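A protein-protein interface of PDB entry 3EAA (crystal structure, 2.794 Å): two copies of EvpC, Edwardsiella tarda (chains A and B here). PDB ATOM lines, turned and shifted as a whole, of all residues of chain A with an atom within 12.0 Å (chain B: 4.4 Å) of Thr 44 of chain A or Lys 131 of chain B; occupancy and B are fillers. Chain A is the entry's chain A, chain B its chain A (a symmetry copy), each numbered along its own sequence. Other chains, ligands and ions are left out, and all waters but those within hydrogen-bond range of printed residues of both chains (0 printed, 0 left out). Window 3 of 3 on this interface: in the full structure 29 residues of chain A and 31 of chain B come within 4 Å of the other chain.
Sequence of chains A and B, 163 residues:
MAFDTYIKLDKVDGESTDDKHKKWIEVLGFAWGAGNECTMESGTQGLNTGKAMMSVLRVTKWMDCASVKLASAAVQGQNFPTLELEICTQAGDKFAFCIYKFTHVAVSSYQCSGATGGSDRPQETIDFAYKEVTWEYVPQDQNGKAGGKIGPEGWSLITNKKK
Of the printed residues of chain B, Thr 44 of chain A touches Lys 131 (2.5 Å). Of the printed residues of chain B, Gln 45 of chain A touches Lys 131 (3.1 Å) and Ile 158 (3.7 Å). Printed residues of chain B within 4 Å of Gly 46 of chain A: Lys 131. Asn 48 of chain A touches none of the printed residues of chain B. No residue of chain A comes within 4 Å of Thr 103 of chain B. Of the printed residues of chain A, His 104 of chain B touches Leu 47 (3.5 Å). No residue of chain A comes within 4 Å of Tyr 130 of chain B. Lys 131 of chain B touches four residues of chain A. No residue of chain A comes within 4 Å of Glu 132 of chain B. Ser 156 of chain B touches none of the printed residues of chain A. The nearest printed residue of chain B that does not touch Thr 44 of chain A is Leu 157 of chain B (4.9 Å). The nearest printed residue of chain B that does not touch Ser 42 of chain A is Lys 131 of chain B (5.4 Å).
The backbone carbonyl oxygen (O) of Thr 44 of chain A sits at hydrogen-bond distance from the side-chain amino group (NZ) of Lys 131 of chain B (2.5 Å). O of Gln 45 of chain A sits close to NZ of Lys 131 of chain B (3.5 Å). O of Gly 46 of chain A is in hydrogen-bond range of NZ of Lys 131 of chain B (2.7 Å).
Leu 157 of chain B touches Ser 42 of chain A (CD2 to CB, 3.8 Å). CG2 of Ile 158 of chain B touches CG of Gln 45 of chain A, at 3.7 Å. Leu 47 of chain A touches His 104 of chain B (CD2 to O, 3.5 Å). CD2 of Leu 47 of chain A touches CG of Lys 131 of chain B, 3.9 Å away.
No position is printed for both chains.
Hydrophobic or aromatic side chains of chain B within 4 Å of the printed part of chain A: Leu 157 and Ile 158. Hydrophobic or aromatic side chains of chain A that line the printed part of chain B: Leu 47. Among the printed residues, no Asp or Glu carboxylate lies within 4 Å of a Lys or Arg side-chain nitrogen of the other chain.
O of Thr 103 of chain B is in hydrogen-bond range of N of Lys 131 of chain B. N of Leu 157 of chain B is in hydrogen-bond range of O of Lys 131 of chain B. The backbone NH (N) of Ile 158 of chain B sits at hydrogen-bond distance from the side-chain hydroxyl (OG) of Ser 156 of chain B (3.0 Å).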
ATOM      1  N   ASN A  36       9.839  19.350  16.279  1.00  0.00           N
ATOM      2  CA  ASN A  36       8.976  20.444  15.882  1.00  0.00           C
ATOM      3  C   ASN A  36       7.897  20.010  14.891  1.00  0.00           C
ATOM      4  O   ASN A  36       7.771  18.830  14.570  1.00  0.00           O
ATOM      5  CB  ASN A  36       9.805  21.603  15.334  1.00  0.00           C
ATOM      6  CG  ASN A  36      10.665  21.200  14.181  1.00  0.00           C
ATOM      7  OD1 ASN A  36      10.197  21.090  13.052  1.00  0.00           O
ATOM      8  ND2 ASN A  36      11.941  20.984  14.452  1.00  0.00           N
ATOM      9  N   GLU A  37       7.098  20.962  14.430  1.00  0.00           N
ATOM     10  CA  GLU A  37       6.019  20.637  13.506  1.00  0.00           C
ATOM     11  C   GLU A  37       6.382  20.939  12.051  1.00  0.00           C
ATOM     12  O   GLU A  37       5.713  21.717  11.365  1.00  0.00           O
ATOM     13  CB  GLU A  37       4.712  21.324  13.918  1.00  0.00           C
ATOM     14  CG  GLU A  37       4.851  22.795  14.287  1.00  0.00           C
ATOM     15  CD  GLU A  37       3.510  23.502  14.373  1.00  0.00           C
ATOM     16  OE1 GLU A  37       3.435  24.676  13.969  1.00  0.00           O
ATOM     17  OE2 GLU A  37       2.531  22.877  14.831  1.00  0.00           O
ATOM     18  N   CYS A  38       7.449  20.293  11.592  1.00  0.00           N
ATOM     19  CA  CYS A  38       7.910  20.432  10.220  1.00  0.00           C
ATOM     20  C   CYS A  38       7.188  19.451   9.307  1.00  0.00           C
ATOM     21  O   CYS A  38       7.374  18.238   9.408  1.00  0.00           O
ATOM     22  CB  CYS A  38       9.422  20.211  10.134  1.00  0.00           C
ATOM     23  SG  CYS A  38      10.149  20.869   8.622  1.00  0.00           S
ATOM     24  N   THR A  39       6.362  19.986   8.415  1.00  0.00           N
ATOM     25  CA  THR A  39       5.576  19.171   7.496  1.00  0.00           C
ATOM     26  C   THR A  39       6.395  18.811   6.261  1.00  0.00           C
ATOM     27  O   THR A  39       7.414  19.434   5.987  1.00  0.00           O
ATOM     28  CB  THR A  39       4.329  19.935   7.028  1.00  0.00           C
ATOM     29  OG1 THR A  39       3.866  20.799   8.074  1.00  0.00           O
ATOM     30  CG2 THR A  39       3.220  18.971   6.622  1.00  0.00           C
ATOM     31  N   MET A  40       5.948  17.808   5.513  1.00  0.00           N
ATOM     32  CA  MET A  40       6.575  17.496   4.232  1.00  0.00           C
ATOM     33  C   MET A  40       5.998  18.409   3.153  1.00  0.00           C
ATOM     34  O   MET A  40       6.270  18.224   1.974  1.00  0.00           O
ATOM     35  CB  MET A  40       6.394  16.024   3.867  1.00  0.00           C
ATOM     36  N   GLU A  41       5.191  19.379   3.590  1.00  0.00           N
ATOM     37  CA  GLU A  41       4.722  20.494   2.777  1.00  0.00           C
ATOM     38  C   GLU A  41       4.466  20.246   1.300  1.00  0.00           C
ATOM     39  O   GLU A  41       3.316  20.066   0.880  1.00  0.00           O
ATOM     40  N   SER A  42       5.542  20.258   0.511  1.00  0.00           N
ATOM     41  CA  SER A  42       5.460  20.060  -0.934  1.00  0.00           C
ATOM     42  C   SER A  42       4.579  21.122  -1.574  1.00  0.00           C
ATOM     43  O   SER A  42       3.696  20.811  -2.372  1.00  0.00           O
ATOM     44  CB  SER A  42       4.942  18.669  -1.259  1.00  0.00           C
ATOM     45  N   GLY A  43       4.835  22.375  -1.211  1.00  0.00           N
ATOM     46  CA  GLY A  43       4.115  23.519  -1.754  1.00  0.00           C
ATOM     47  C   GLY A  43       4.717  24.837  -1.249  1.00  0.00           C
ATOM     48  O   GLY A  43       4.558  25.880  -1.880  1.00  0.00           O
ATOM     49  N   THR A  44       5.407  24.780  -0.111  1.00  0.00           N
ATOM     50  CA  THR A  44       6.027  25.966   0.482  1.00  0.00           C
ATOM     51  C   THR A  44       7.535  26.011   0.228  1.00  0.00           C
ATOM     52  O   THR A  44       8.200  24.980   0.233  1.00  0.00           O
ATOM     53  CB  THR A  44       5.729  26.035   1.976  1.00  0.00           C
ATOM     54  N   GLN A  45       8.069  27.211   0.025  1.00  0.00           N
ATOM     55  CA  GLN A  45       9.464  27.368  -0.386  1.00  0.00           C
ATOM     56  C   GLN A  45      10.454  27.162   0.761  1.00  0.00           C
ATOM     57  O   GLN A  45      11.415  26.400   0.636  1.00  0.00           O
ATOM     58  CB  GLN A  45       9.679  28.735  -1.048  1.00  0.00           C
ATOM     59  CG  GLN A  45      10.887  28.806  -1.976  1.00  0.00           C
ATOM     60  CD  GLN A  45      12.192  28.885  -1.213  1.00  0.00           C
ATOM     61  OE1 GLN A  45      12.204  29.172  -0.017  1.00  0.00           O
ATOM     62  NE2 GLN A  45      13.301  28.638  -1.902  1.00  0.00           N
ATOM     63  N   GLY A  46      10.229  27.854   1.874  1.00  0.00           N
ATOM     64  CA  GLY A  46      11.038  27.653   3.062  1.00  0.00           C
ATOM     65  C   GLY A  46      10.694  26.318   3.696  1.00  0.00           C
ATOM     66  O   GLY A  46       9.819  25.607   3.198  1.00  0.00           O
ATOM     67  N   LEU A  47      11.374  25.965   4.783  1.00  0.00           N
ATOM     68  CA  LEU A  47      11.076  24.717   5.467  1.00  0.00           C
ATOM     69  C   LEU A  47       9.781  24.826   6.266  1.00  0.00           C
ATOM     70  O   LEU A  47       8.850  24.042   6.052  1.00  0.00           O
ATOM     71  CB  LEU A  47      12.221  24.303   6.381  1.00  0.00           C
ATOM     72  CG  LEU A  47      13.312  23.432   5.760  1.00  0.00           C
ATOM     73  CD1 LEU A  47      14.306  22.996   6.830  1.00  0.00           C
ATOM     74  CD2 LEU A  47      12.709  22.231   5.058  1.00  0.00           C
ATOM     75  N   ASN A  48       9.735  25.798   7.180  1.00  0.00           N
ATOM     76  CA  ASN A  48       8.553  26.051   8.011  1.00  0.00           C
ATOM     77  C   ASN A  48       8.474  25.107   9.205  1.00  0.00           C
ATOM     78  O   ASN A  48       7.629  24.215   9.251  1.00  0.00           O
ATOM     79  CB  ASN A  48       7.266  25.984   7.183  1.00  0.00           C
ATOM     80  N   THR A  49       9.354  25.344  10.174  1.00  0.00           N
ATOM     81  CA  THR A  49       9.496  24.509  11.363  1.00  0.00           C
ATOM     82  C   THR A  49       8.346  24.670  12.352  1.00  0.00           C
ATOM     83  O   THR A  49       8.067  23.770  13.155  1.00  0.00           O
ATOM     84  CB  THR A  49      10.792  24.840  12.114  1.00  0.00           C
ATOM     85  OG1 THR A  49      10.946  23.932  13.204  1.00  0.00           O
ATOM     86  CG2 THR A  49      10.739  26.253  12.665  1.00  0.00           C
ATOM     87  N   GLY A  50       7.693  25.825  12.301  1.00  0.00           N
ATOM     88  CA  GLY A  50       6.601  26.110  13.208  1.00  0.00           C
ATOM     89  C   GLY A  50       7.039  26.079  14.658  1.00  0.00           C
ATOM     90  O   GLY A  50       8.087  26.620  15.012  1.00  0.00           O
ATOM     91  N   THR B 103      18.941  17.918   0.636  1.00  0.00           N
ATOM     92  CA  THR B 103      19.308  19.316   0.570  1.00  0.00           C
ATOM     93  C   THR B 103      18.239  20.122   1.283  1.00  0.00           C
ATOM     94  O   THR B 103      17.055  19.944   1.022  1.00  0.00           O
ATOM     95  CB  THR B 103      19.421  19.786  -0.906  1.00  0.00           C
ATOM     96  OG1 THR B 103      20.000  18.750  -1.706  1.00  0.00           O
ATOM     97  CG2 THR B 103      20.277  21.029  -1.025  1.00  0.00           C
ATOM     98  N   HIS B 104      18.660  21.005   2.182  1.00  0.00           N
ATOM     99  CA  HIS B 104      17.739  21.808   2.992  1.00  0.00           C
ATOM    100  C   HIS B 104      17.035  20.964   4.063  1.00  0.00           C
ATOM    101  O   HIS B 104      15.809  20.880   4.120  1.00  0.00           O
ATOM    102  CB  HIS B 104      16.738  22.568   2.114  1.00  0.00           C
ATOM    103  CG  HIS B 104      17.384  23.514   1.158  1.00  0.00           C
ATOM    104  ND1 HIS B 104      17.979  24.704   1.567  1.00  0.00           N
ATOM    105  CD2 HIS B 104      17.563  23.464  -0.180  1.00  0.00           C
ATOM    106  CE1 HIS B 104      18.480  25.323   0.527  1.00  0.00           C
ATOM    107  NE2 HIS B 104      18.243  24.594  -0.559  1.00  0.00           N
ATOM    108  N   TYR B 130      13.111  17.437   4.825  1.00  0.00           N
ATOM    109  CA  TYR B 130      14.001  17.967   3.784  1.00  0.00           C
ATOM    110  C   TYR B 130      13.271  18.671   2.633  1.00  0.00           C
ATOM    111  O   TYR B 130      12.051  18.809   2.648  1.00  0.00           O
ATOM    112  CB  TYR B 130      14.913  16.853   3.238  1.00  0.00           C
ATOM    113  CG  TYR B 130      14.191  15.598   2.774  1.00  0.00           C
ATOM    114  CD1 TYR B 130      13.570  14.743   3.683  1.00  0.00           C
ATOM    115  CD2 TYR B 130      14.148  15.261   1.429  1.00  0.00           C
ATOM    116  CE1 TYR B 130      12.922  13.604   3.258  1.00  0.00           C
ATOM    117  CE2 TYR B 130      13.501  14.121   0.998  1.00  0.00           C
ATOM    118  CZ  TYR B 130      12.892  13.300   1.913  1.00  0.00           C
ATOM    119  OH  TYR B 130      12.248  12.167   1.472  1.00  0.00           O
ATOM    120  N   LYS B 131      14.029  19.127   1.640  1.00  0.00           N
ATOM    121  CA  LYS B 131      13.441  19.775   0.471  1.00  0.00           C
ATOM    122  C   LYS B 131      13.749  19.002  -0.802  1.00  0.00           C
ATOM    123  O   LYS B 131      12.897  18.886  -1.683  1.00  0.00           O
ATOM    124  CB  LYS B 131      13.943  21.212   0.326  1.00  0.00           C
ATOM    125  CG  LYS B 131      13.261  22.211   1.243  1.00  0.00           C
ATOM    126  CD  LYS B 131      11.778  22.313   0.953  1.00  0.00           C
ATOM    127  CE  LYS B 131      11.161  23.467   1.720  1.00  0.00           C
ATOM    128  NZ  LYS B 131       9.688  23.520   1.565  1.00  0.00           N
ATOM    129  N   GLU B 132      14.970  18.481  -0.898  1.00  0.00           N
ATOM    130  CA  GLU B 132      15.426  17.819  -2.115  1.00  0.00           C
ATOM    131  C   GLU B 132      16.300  16.605  -1.799  1.00  0.00           C
ATOM    132  O   GLU B 132      16.764  16.450  -0.677  1.00  0.00           O
ATOM    133  CB  GLU B 132      16.178  18.815  -3.000  1.00  0.00           C
ATOM    134  CG  GLU B 132      15.322  19.981  -3.485  1.00  0.00           C
ATOM    135  CD  GLU B 132      16.114  21.001  -4.284  1.00  0.00           C
ATOM    136  OE1 GLU B 132      17.303  21.224  -3.968  1.00  0.00           O
ATOM    137  OE2 GLU B 132      15.545  21.591  -5.224  1.00  0.00           O
ATOM    138  N   SER B 156      12.720  17.359  -6.378  1.00  0.00           N
ATOM    139  CA  SER B 156      12.634  18.545  -5.529  1.00  0.00           C
ATOM    140  C   SER B 156      11.208  18.943  -5.226  1.00  0.00           C
ATOM    141  O   SER B 156      10.393  19.079  -6.130  1.00  0.00           O
ATOM    142  CB  SER B 156      13.313  19.735  -6.192  1.00  0.00           C
ATOM    143  OG  SER B 156      12.963  20.946  -5.537  1.00  0.00           O
ATOM    144  N   LEU B 157      10.929  19.178  -3.949  1.00  0.00           N
ATOM    145  CA  LEU B 157       9.615  19.612  -3.500  1.00  0.00           C
ATOM    146  C   LEU B 157       9.434  21.117  -3.616  1.00  0.00           C
ATOM    147  O   LEU B 157       8.361  21.639  -3.316  1.00  0.00           O
ATOM    148  CB  LEU B 157       9.382  19.170  -2.057  1.00  0.00           C
ATOM    149  CG  LEU B 157       9.342  17.655  -1.856  1.00  0.00           C
ATOM    150  CD1 LEU B 157       9.374  17.299  -0.378  1.00  0.00           C
ATOM    151  CD2 LEU B 157       8.121  17.053  -2.548  1.00  0.00           C
ATOM    152  N   ILE B 158      10.478  21.819  -4.049  1.00  0.00           N
ATOM    153  CA  ILE B 158      10.344  23.249  -4.281  1.00  0.00           C
ATOM    154  C   ILE B 158       9.891  23.513  -5.720  1.00  0.00           C
ATOM    155  O   ILE B 158       9.237  24.515  -6.004  1.00  0.00           O
ATOM    156  CB  ILE B 158      11.654  24.019  -4.008  1.00  0.00           C
ATOM    157  CG1 ILE B 158      12.541  23.277  -3.011  1.00  0.00           C
ATOM    158  CG2 ILE B 158      11.349  25.412  -3.489  1.00  0.00           C
ATOM    159  CD1 ILE B 158      13.758  24.081  -2.585  1.00  0.00           C
